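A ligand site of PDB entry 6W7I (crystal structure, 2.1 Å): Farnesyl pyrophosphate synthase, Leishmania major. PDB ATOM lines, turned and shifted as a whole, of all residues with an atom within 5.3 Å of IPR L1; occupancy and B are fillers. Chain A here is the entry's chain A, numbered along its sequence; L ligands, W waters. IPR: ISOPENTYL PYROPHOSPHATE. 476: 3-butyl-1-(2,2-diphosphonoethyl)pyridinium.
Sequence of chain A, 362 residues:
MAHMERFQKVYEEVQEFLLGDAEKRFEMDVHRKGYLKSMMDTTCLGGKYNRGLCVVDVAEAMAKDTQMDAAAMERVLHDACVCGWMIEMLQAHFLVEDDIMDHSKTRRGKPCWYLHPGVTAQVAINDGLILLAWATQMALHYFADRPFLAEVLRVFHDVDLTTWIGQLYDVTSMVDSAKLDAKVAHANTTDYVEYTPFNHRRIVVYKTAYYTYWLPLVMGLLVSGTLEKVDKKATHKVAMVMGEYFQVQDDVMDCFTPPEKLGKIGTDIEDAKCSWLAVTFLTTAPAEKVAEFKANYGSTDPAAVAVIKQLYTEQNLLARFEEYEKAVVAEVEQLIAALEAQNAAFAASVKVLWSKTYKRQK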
ATOM      1  N   GLY A  46       0.476 -18.870  13.216  1.00  0.00           N
ATOM      2  CA  GLY A  46       0.706 -19.378  14.562  1.00  0.00           C
ATOM      3  C   GLY A  46      -0.379 -20.319  15.063  1.00  0.00           C
ATOM      4  O   GLY A  46      -0.182 -21.023  16.058  1.00  0.00           O
ATOM      5  N   GLY A  47      -1.517 -20.343  14.381  1.00  0.00           N
ATOM      6  CA  GLY A  47      -2.654 -21.184  14.770  1.00  0.00           C
ATOM      7  C   GLY A  47      -2.591 -22.532  14.095  1.00  0.00           C
ATOM      8  O   GLY A  47      -1.569 -22.876  13.491  1.00  0.00           O
ATOM      9  N   LYS A  48      -3.682 -23.299  14.175  1.00  0.00           N
ATOM     10  CA  LYS A  48      -3.726 -24.670  13.651  1.00  0.00           C
ATOM     11  C   LYS A  48      -4.080 -24.726  12.168  1.00  0.00           C
ATOM     12  O   LYS A  48      -3.873 -25.733  11.500  1.00  0.00           O
ATOM     13  CB  LYS A  48      -4.716 -25.528  14.450  1.00  0.00           C
ATOM     14  CG  LYS A  48      -4.414 -25.657  15.945  1.00  0.00           C
ATOM     15  CD  LYS A  48      -5.472 -26.496  16.708  1.00  0.00           C
ATOM     16  CE  LYS A  48      -6.748 -25.690  17.020  1.00  0.00           C
ATOM     17  NZ  LYS A  48      -6.513 -24.651  18.086  1.00  0.00           N
ATOM     18  N   TYR A  49      -4.629 -23.623  11.652  1.00  0.00           N
ATOM     19  CA  TYR A  49      -5.139 -23.529  10.277  1.00  0.00           C
ATOM     20  C   TYR A  49      -6.251 -24.538   9.947  1.00  0.00           C
ATOM     21  O   TYR A  49      -6.447 -24.874   8.782  1.00  0.00           O
ATOM     22  CB  TYR A  49      -4.001 -23.587   9.240  1.00  0.00           C
ATOM     23  CG  TYR A  49      -2.832 -22.699   9.557  1.00  0.00           C
ATOM     24  CD1 TYR A  49      -2.869 -21.330   9.277  1.00  0.00           C
ATOM     25  CD2 TYR A  49      -1.682 -23.211  10.160  1.00  0.00           C
ATOM     26  CE1 TYR A  49      -1.808 -20.504   9.577  1.00  0.00           C
ATOM     27  CE2 TYR A  49      -0.597 -22.385  10.466  1.00  0.00           C
ATOM     28  CZ  TYR A  49      -0.669 -21.033  10.160  1.00  0.00           C
ATOM     29  OH  TYR A  49       0.397 -20.221  10.458  1.00  0.00           O
ATOM     30  N   ARG A  51      -9.477 -24.114   9.922  1.00  0.00           N
ATOM     31  CA  ARG A  51     -10.491 -23.481   9.069  1.00  0.00           C
ATOM     32  C   ARG A  51     -10.052 -23.330   7.617  1.00  0.00           C
ATOM     33  O   ARG A  51     -10.772 -23.733   6.701  1.00  0.00           O
ATOM     34  CB  ARG A  51     -10.925 -22.114   9.644  1.00  0.00           C
ATOM     35  CG  ARG A  51     -11.656 -22.181  10.978  1.00  0.00           C
ATOM     36  CD  ARG A  51     -11.808 -20.805  11.602  1.00  0.00           C
ATOM     37  NE  ARG A  51     -12.212 -20.871  13.005  1.00  0.00           N
ATOM     38  CZ  ARG A  51     -11.389 -21.080  14.031  1.00  0.00           C
ATOM     39  NH1 ARG A  51     -10.088 -21.258  13.842  1.00  0.00           N
ATOM     40  NH2 ARG A  51     -11.871 -21.131  15.266  1.00  0.00           N
ATOM     41  N   GLU A  88      -9.125 -17.455   7.652  1.00  0.00           N
ATOM     42  CA  GLU A  88      -8.025 -17.291   8.582  1.00  0.00           C
ATOM     43  C   GLU A  88      -7.868 -15.822   8.940  1.00  0.00           C
ATOM     44  O   GLU A  88      -7.566 -15.487  10.084  1.00  0.00           O
ATOM     45  CB  GLU A  88      -6.722 -17.864   8.023  1.00  0.00           C
ATOM     46  CG  GLU A  88      -6.685 -19.400   7.988  1.00  0.00           C
ATOM     47  CD  GLU A  88      -6.853 -20.043   9.346  1.00  0.00           C
ATOM     48  OE1 GLU A  88      -6.382 -19.461  10.350  1.00  0.00           O
ATOM     49  OE2 GLU A  88      -7.452 -21.137   9.409  1.00  0.00           O
ATOM     50  N   GLN A  91     -10.813 -15.004  11.216  1.00  0.00           N
ATOM     51  CA  GLN A  91     -10.344 -15.492  12.508  1.00  0.00           C
ATOM     52  C   GLN A  91      -9.379 -14.503  13.140  1.00  0.00           C
ATOM     53  O   GLN A  91      -9.523 -14.185  14.308  1.00  0.00           O
ATOM     54  CB  GLN A  91      -9.670 -16.872  12.355  1.00  0.00           C
ATOM     55  CG  GLN A  91      -8.836 -17.351  13.577  1.00  0.00           C
ATOM     56  CD  GLN A  91      -9.685 -17.907  14.718  1.00  0.00           C
ATOM     57  OE1 GLN A  91      -9.291 -18.860  15.392  1.00  0.00           O
ATOM     58  NE2 GLN A  91     -10.849 -17.309  14.935  1.00  0.00           N
ATOM     59  N   LEU A  95      -9.937 -12.533  16.793  1.00  0.00           N
ATOM     60  CA  LEU A  95      -9.095 -12.731  17.971  1.00  0.00           C
ATOM     61  C   LEU A  95      -8.424 -11.440  18.426  1.00  0.00           C
ATOM     62  O   LEU A  95      -8.321 -11.184  19.621  1.00  0.00           O
ATOM     63  CB  LEU A  95      -8.082 -13.874  17.757  1.00  0.00           C
ATOM     64  CG  LEU A  95      -8.600 -15.229  17.266  1.00  0.00           C
ATOM     65  CD1 LEU A  95      -7.473 -16.272  17.265  1.00  0.00           C
ATOM     66  CD2 LEU A  95      -9.802 -15.737  18.101  1.00  0.00           C
ATOM     67  N   ARG A 107      -1.683 -14.880  23.044  1.00  0.00           N
ATOM     68  CA  ARG A 107      -2.351 -15.451  21.896  1.00  0.00           C
ATOM     69  C   ARG A 107      -1.316 -16.242  21.110  1.00  0.00           C
ATOM     70  O   ARG A 107      -0.276 -15.686  20.720  1.00  0.00           O
ATOM     71  CB  ARG A 107      -2.983 -14.359  21.006  1.00  0.00           C
ATOM     72  CG  ARG A 107      -3.677 -14.884  19.714  1.00  0.00           C
ATOM     73  CD  ARG A 107      -4.788 -15.908  20.017  1.00  0.00           C
ATOM     74  NE  ARG A 107      -5.991 -15.279  20.573  1.00  0.00           N
ATOM     75  CZ  ARG A 107      -7.088 -15.941  20.952  1.00  0.00           C
ATOM     76  NH1 ARG A 107      -7.175 -17.271  20.830  1.00  0.00           N
ATOM     77  NH2 ARG A 107      -8.127 -15.272  21.429  1.00  0.00           N
ATOM     78  N   ARG A 108      -1.605 -17.527  20.898  1.00  0.00           N
ATOM     79  CA  ARG A 108      -0.727 -18.426  20.152  1.00  0.00           C
ATOM     80  C   ARG A 108       0.721 -18.379  20.695  1.00  0.00           C
ATOM     81  O   ARG A 108       1.692 -18.438  19.937  1.00  0.00           O
ATOM     82  CB  ARG A 108      -0.809 -18.109  18.645  1.00  0.00           C
ATOM     83  CG  ARG A 108      -2.179 -18.415  17.999  1.00  0.00           C
ATOM     84  CD  ARG A 108      -2.385 -17.657  16.684  1.00  0.00           C
ATOM     85  NE  ARG A 108      -3.685 -17.939  16.057  1.00  0.00           N
ATOM     86  CZ  ARG A 108      -4.175 -17.284  14.992  1.00  0.00           C
ATOM     87  NH1 ARG A 108      -3.489 -16.302  14.419  1.00  0.00           N
ATOM     88  NH2 ARG A 108      -5.361 -17.606  14.493  1.00  0.00           N
ATOM     89  N   THR A 208     -19.182 -19.524  17.490  1.00  0.00           N
ATOM     90  CA  THR A 208     -18.151 -20.473  17.058  1.00  0.00           C
ATOM     91  C   THR A 208     -18.504 -21.384  15.874  1.00  0.00           C
ATOM     92  O   THR A 208     -17.754 -21.452  14.902  1.00  0.00           O
ATOM     93  CB  THR A 208     -17.610 -21.294  18.259  1.00  0.00           C
ATOM     94  OG1 THR A 208     -16.972 -20.401  19.181  1.00  0.00           O
ATOM     95  CG2 THR A 208     -16.586 -22.360  17.816  1.00  0.00           C
ATOM     96  N   TYR A 211     -18.641 -19.978  11.941  1.00  0.00           N
ATOM     97  CA  TYR A 211     -17.371 -19.601  11.293  1.00  0.00           C
ATOM     98  C   TYR A 211     -16.290 -20.679  11.298  1.00  0.00           C
ATOM     99  O   TYR A 211     -15.432 -20.697  10.412  1.00  0.00           O
ATOM    100  CB  TYR A 211     -16.838 -18.252  11.812  1.00  0.00           C
ATOM    101  CG  TYR A 211     -15.829 -18.249  12.968  1.00  0.00           C
ATOM    102  CD1 TYR A 211     -16.249 -18.264  14.308  1.00  0.00           C
ATOM    103  CD2 TYR A 211     -14.457 -18.141  12.713  1.00  0.00           C
ATOM    104  CE1 TYR A 211     -15.320 -18.214  15.371  1.00  0.00           C
ATOM    105  CE2 TYR A 211     -13.536 -18.099  13.757  1.00  0.00           C
ATOM    106  CZ  TYR A 211     -13.965 -18.131  15.086  1.00  0.00           C
ATOM    107  OH  TYR A 211     -13.022 -18.076  16.107  1.00  0.00           O
ATOM    108  N   THR A 212     -16.339 -21.571  12.289  1.00  0.00           N
ATOM    109  CA  THR A 212     -15.325 -22.612  12.414  1.00  0.00           C
ATOM    110  C   THR A 212     -15.660 -23.898  11.638  1.00  0.00           C
ATOM    111  O   THR A 212     -14.761 -24.573  11.146  1.00  0.00           O
ATOM    112  CB  THR A 212     -15.008 -22.888  13.900  1.00  0.00           C
ATOM    113  OG1 THR A 212     -14.790 -21.626  14.553  1.00  0.00           O
ATOM    114  CG2 THR A 212     -13.752 -23.751  14.078  1.00  0.00           C
ATOM    115  N   PHE A 246     -16.649 -28.349  19.649  1.00  0.00           N
ATOM    116  CA  PHE A 246     -15.365 -27.654  19.575  1.00  0.00           C
ATOM    117  C   PHE A 246     -15.244 -26.566  20.638  1.00  0.00           C
ATOM    118  O   PHE A 246     -14.167 -26.406  21.244  1.00  0.00           O
ATOM    119  CB  PHE A 246     -15.158 -27.059  18.183  1.00  0.00           C
ATOM    120  CG  PHE A 246     -13.851 -26.327  18.006  1.00  0.00           C
ATOM    121  CD1 PHE A 246     -12.708 -27.009  17.569  1.00  0.00           C
ATOM    122  CD2 PHE A 246     -13.764 -24.946  18.226  1.00  0.00           C
ATOM    123  CE1 PHE A 246     -11.509 -26.340  17.375  1.00  0.00           C
ATOM    124  CE2 PHE A 246     -12.558 -24.269  18.042  1.00  0.00           C
ATOM    125  CZ  PHE A 246     -11.431 -24.966  17.616  1.00  0.00           C
ATOM    126  N   GLN A 247     -16.316 -25.801  20.854  1.00  0.00           N
ATOM    127  CA  GLN A 247     -16.315 -24.738  21.877  1.00  0.00           C
ATOM    128  C   GLN A 247     -16.379 -25.275  23.297  1.00  0.00           C
ATOM    129  O   GLN A 247     -15.788 -24.698  24.206  1.00  0.00           O
ATOM    130  CB  GLN A 247     -17.438 -23.713  21.649  1.00  0.00           C
ATOM    131  CG  GLN A 247     -17.307 -22.418  22.486  1.00  0.00           C
ATOM    132  CD  GLN A 247     -15.960 -21.725  22.307  1.00  0.00           C
ATOM    133  OE1 GLN A 247     -15.516 -21.487  21.191  1.00  0.00           O
ATOM    134  NE2 GLN A 247     -15.315 -21.383  23.436  1.00  0.00           N
ATOM    135  N   ASP A 250     -12.901 -26.017  24.059  1.00  0.00           N
ATOM    136  CA  ASP A 250     -12.229 -24.755  24.378  1.00  0.00           C
ATOM    137  C   ASP A 250     -12.546 -24.305  25.798  1.00  0.00           C
ATOM    138  O   ASP A 250     -11.651 -23.875  26.519  1.00  0.00           O
ATOM    139  CB  ASP A 250     -12.625 -23.675  23.380  1.00  0.00           C
ATOM    140  CG  ASP A 250     -11.750 -22.440  23.483  1.00  0.00           C
ATOM    141  OD1 ASP A 250     -10.556 -22.515  23.130  1.00  0.00           O
ATOM    142  OD2 ASP A 250     -12.273 -21.380  23.900  1.00  0.00           O
ATOM    143  N   LYS A 264      -2.493 -19.583  25.260  1.00  0.00           N
ATOM    144  CA  LYS A 264      -3.339 -18.473  25.673  1.00  0.00           C
ATOM    145  C   LYS A 264      -3.729 -18.644  27.134  1.00  0.00           C
ATOM    146  O   LYS A 264      -3.749 -19.777  27.644  1.00  0.00           O
ATOM    147  CB  LYS A 264      -4.587 -18.369  24.770  1.00  0.00           C
ATOM    148  CG  LYS A 264      -5.495 -19.592  24.787  1.00  0.00           C
ATOM    149  CD  LYS A 264      -6.483 -19.625  23.634  1.00  0.00           C
ATOM    150  CE  LYS A 264      -7.500 -20.763  23.836  1.00  0.00           C
ATOM    151  NZ  LYS A 264      -8.588 -20.757  22.799  1.00  0.00           N
ATOM    152  N   ARG A 360      -9.010 -33.410  20.400  1.00  0.00           N
ATOM    153  CA  ARG A 360      -7.870 -32.498  20.181  1.00  0.00           C
ATOM    154  C   ARG A 360      -7.370 -32.023  21.537  1.00  0.00           C
ATOM    155  O   ARG A 360      -8.124 -32.040  22.501  1.00  0.00           O
ATOM    156  CB  ARG A 360      -8.261 -31.292  19.308  1.00  0.00           C
ATOM    157  CG  ARG A 360      -9.144 -30.248  20.009  1.00  0.00           C
ATOM    158  CD  ARG A 360      -9.820 -29.288  19.022  1.00  0.00           C
ATOM    159  NE  ARG A 360     -10.744 -28.401  19.735  1.00  0.00           N
ATOM    160  CZ  ARG A 360     -10.415 -27.227  20.265  1.00  0.00           C
ATOM    161  NH1 ARG A 360      -9.181 -26.737  20.158  1.00  0.00           N
ATOM    162  NH2 ARG A 360     -11.352 -26.506  20.891  1.00  0.00           N
ATOM    163  N   LYS A 362      -5.311 -29.026  21.880  1.00  0.00           N
ATOM    164  CA  LYS A 362      -5.089 -27.576  21.846  1.00  0.00           C
ATOM    165  C   LYS A 362      -5.835 -26.941  20.675  1.00  0.00           C
ATOM    166  O   LYS A 362      -5.907 -25.723  20.560  1.00  0.00           O
ATOM    167  CB  LYS A 362      -3.587 -27.234  21.774  1.00  0.00           C
ATOM    168  CG  LYS A 362      -2.882 -27.690  20.503  1.00  0.00           C
ATOM    169  CD  LYS A 362      -1.504 -27.010  20.338  1.00  0.00           C
ATOM    170  CE  LYS A 362      -1.664 -25.604  19.758  1.00  0.00           C
ATOM    171  NZ  LYS A 362      -0.387 -25.047  19.199  1.00  0.00           N
ATOM    172  OXT LYS A 362      -6.387 -27.644  19.828  1.00  0.00           O
HETATM  173  P11 IPR L   1      -6.239 -20.976  16.175  1.00  0.00           P
HETATM  174  O14 IPR L   1      -6.804 -20.147  15.050  1.00  0.00           O
HETATM  175  O12 IPR L   1      -5.142 -20.274  16.936  1.00  0.00           O
HETATM  176  O13 IPR L   1      -6.016 -22.420  15.786  1.00  0.00           O
HETATM  177  O10 IPR L   1      -7.383 -20.995  17.327  1.00  0.00           O
HETATM  178  P7  IPR L   1      -8.727 -21.893  17.412  1.00  0.00           P
HETATM  179  O8  IPR L   1      -9.047 -22.510  16.079  1.00  0.00           O
HETATM  180  O9  IPR L   1      -8.586 -22.816  18.599  1.00  0.00           O
HETATM  181  O6  IPR L   1      -9.883 -20.812  17.740  1.00  0.00           O
HETATM  182  C5  IPR L   1      -9.795 -19.874  18.835  1.00  0.00           C
HETATM  183  C4  IPR L   1     -11.187 -19.323  19.153  1.00  0.00           C
HETATM  184  C2  IPR L   1     -12.213 -20.423  19.298  1.00  0.00           C
HETATM  185  C1  IPR L   1     -13.271 -20.603  18.246  1.00  0.00           C
HETATM  186  C3  IPR L   1     -12.203 -21.255  20.336  1.00  0.00           C
HETATM  187  O11 476 L   2     -10.538 -18.713  24.303  1.00  0.00           O
HETATM  188  P10 476 L   2     -10.429 -17.735  23.176  1.00  0.00           P
HETATM  189  O13 476 L   2      -9.700 -18.290  21.993  1.00  0.00           O
HETATM  190  O12 476 L   2      -9.945 -16.362  23.542  1.00  0.00           O
HETATM  191  C8  476 L   2     -12.158 -17.542  22.569  1.00  0.00           C
HETATM  192  P9  476 L   2     -13.404 -17.161  23.845  1.00  0.00           P
HETATM  193  O15 476 L   2     -13.048 -15.804  24.399  1.00  0.00           O
HETATM  194  O14 476 L   2     -13.374 -18.294  24.847  1.00  0.00           O
HETATM  195  O16 476 L   2     -14.743 -17.143  23.134  1.00  0.00           O
HETATM  196  C7  476 L   2     -12.215 -16.451  21.486  1.00  0.00           C
HETATM  197  N2  476 L   2     -13.372 -16.560  20.593  1.00  0.00           N
HETATM  198  C1  476 L   2     -13.863 -15.447  19.976  1.00  0.00           C
HETATM  199  C6  476 L   2     -14.958 -15.550  19.102  1.00  0.00           C
HETATM  200  C5  476 L   2     -15.561 -16.777  18.866  1.00  0.00           C
HETATM  201  C4  476 L   2     -15.050 -17.898  19.489  1.00  0.00           C
HETATM  202  C3  476 L   2     -13.951 -17.754  20.356  1.00  0.00           C
HETATM  203  C17 476 L   2     -15.582 -14.378  18.384  1.00  0.00           C
HETATM  204  C18 476 L   2     -14.850 -13.062  18.533  1.00  0.00           C
HETATM  205  C19 476 L   2     -15.754 -11.960  17.974  1.00  0.00           C
HETATM  206  C20 476 L   2     -14.989 -10.669  18.124  1.00  0.00           C
HETATM  207  O   HOH W   1      -6.937 -21.681  20.640  1.00  0.00           O
HETATM  208  O   HOH W   2      -9.819 -23.879  21.073  1.00  0.00           O
HETATM  209  O   HOH W   3      -9.767 -24.719  14.800  1.00  0.00           O
HETATM  210  O   HOH W   4      -5.764 -19.600  19.524  1.00  0.00           O
HETATM  211  O   HOH W   5      -7.335 -23.541  13.662  1.00  0.00           O
HETATM  212  O   HOH W   6      -5.531 -20.785  12.616  1.00  0.00           O
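The guanidinium group (NH1) of Arg 51 lies within salt-bridge range of an oxygen (O8) of IPR L1. The backbone NH (N) of Lys 48 is in hydrogen-bond range of an oxygen (O13) of IPR L1 (3.0 Å). O9 of IPR L1 lies within salt-bridge range of NZ of Lys 48, 2.8 Å away. The side-chain amide oxygen (OE1) of Gln 91 sits close to an oxygen (O14) of IPR L1. An oxygen (O12) of IPR L1 lies within salt-bridge range of the guanidinium group (NE) of Arg 108, 2.9 Å away. An oxygen (O13) of 476 L2 lies within salt-bridge range of the guanidinium group of Arg 107. An oxygen (O13) of 476 L2 lies within salt-bridge range of the side-chain amino group (NZ) of Lys 264 (2.8 Å).
NH1 of Arg 51 sits at hydrogen-bond distance from OE1 of Gln 91 (3.0 Å). The guanidinium group (NH2) of Arg 51 lies within hydrogen-bond range of the side-chain hydroxyl (OH) of Tyr 211 (3.4 Å). The guanidinium group of Arg 51 sits at hydrogen-bond distance from the side-chain hydroxyl of Thr 212, 3.0 Å away. The side-chain amino group (NZ) of Lys 48 lies within salt-bridge range of the chain-end carboxylate (O) of Lys 362, 2.8 Å away. The side-chain amide nitrogen of Gln 91 sits at hydrogen-bond distance from the side-chain hydroxyl of Tyr 211, at 2.6 Å. The side-chain carboxylate (OD2) of Asp 250 sits close to the side-chain amide nitrogen (NE2) of Gln 247, at 3.1 Å. The side-chain carboxylate (OD1) of Asp 250 lies within salt-bridge range of the side-chain amino group (NZ) of Lys 264. NH2 of Arg 360 is in hydrogen-bond range of O of Phe 246, at 2.8 Å.
Gly 47 touches IPR L1 (CA to O12, 3.4 Å). Leu 95 touches IPR L1 (CD2 to C4, 3.99 Å). Thr 208 touches IPR L1. OH of Tyr 211 touches C1 of IPR L1, at 3.3 Å. CZ of Phe 246 touches O9 of IPR L1 (3.7 Å). Gln 247 touches IPR L1. Asp 250 touches IPR L1 (CG to C3, 3.4 Å). Hydrophobic or aromatic side chains that line IPR L1: Leu 95 and Phe 246. Of the 19 residues printed, 11 come within 4 Å of IPR L1. The nearest printed residue that does not touch IPR L1 is Thr 212 (4.1 Å).
Water W5 bridges O13 of IPR L1 (2.7 Å) and N of Tyr 49 (3.4 Å). Water W4 lies within hydrogen-bond range of O12 of IPR L1 (2.7 Å) and NH1 of Arg 107 (3.0 Å). Water W6 lies within hydrogen-bond range of the side-chain carboxylate (OE1) of Glu 88, an oxygen (O14) of IPR L1, the backbone NH (N) of Tyr 49 and the backbone NH (N) of Lys 48. Water W1 bridges an oxygen (O9) of IPR L1 (2.9 Å) and the side-chain amino group of Lys 264 (2.9 Å). Water W2 lies within hydrogen-bond range of OD1 of Asp 250 (2.6 Å), O9 of IPR L1 (3.0 Å) and NH2 of Arg 360 (3.0 Å).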
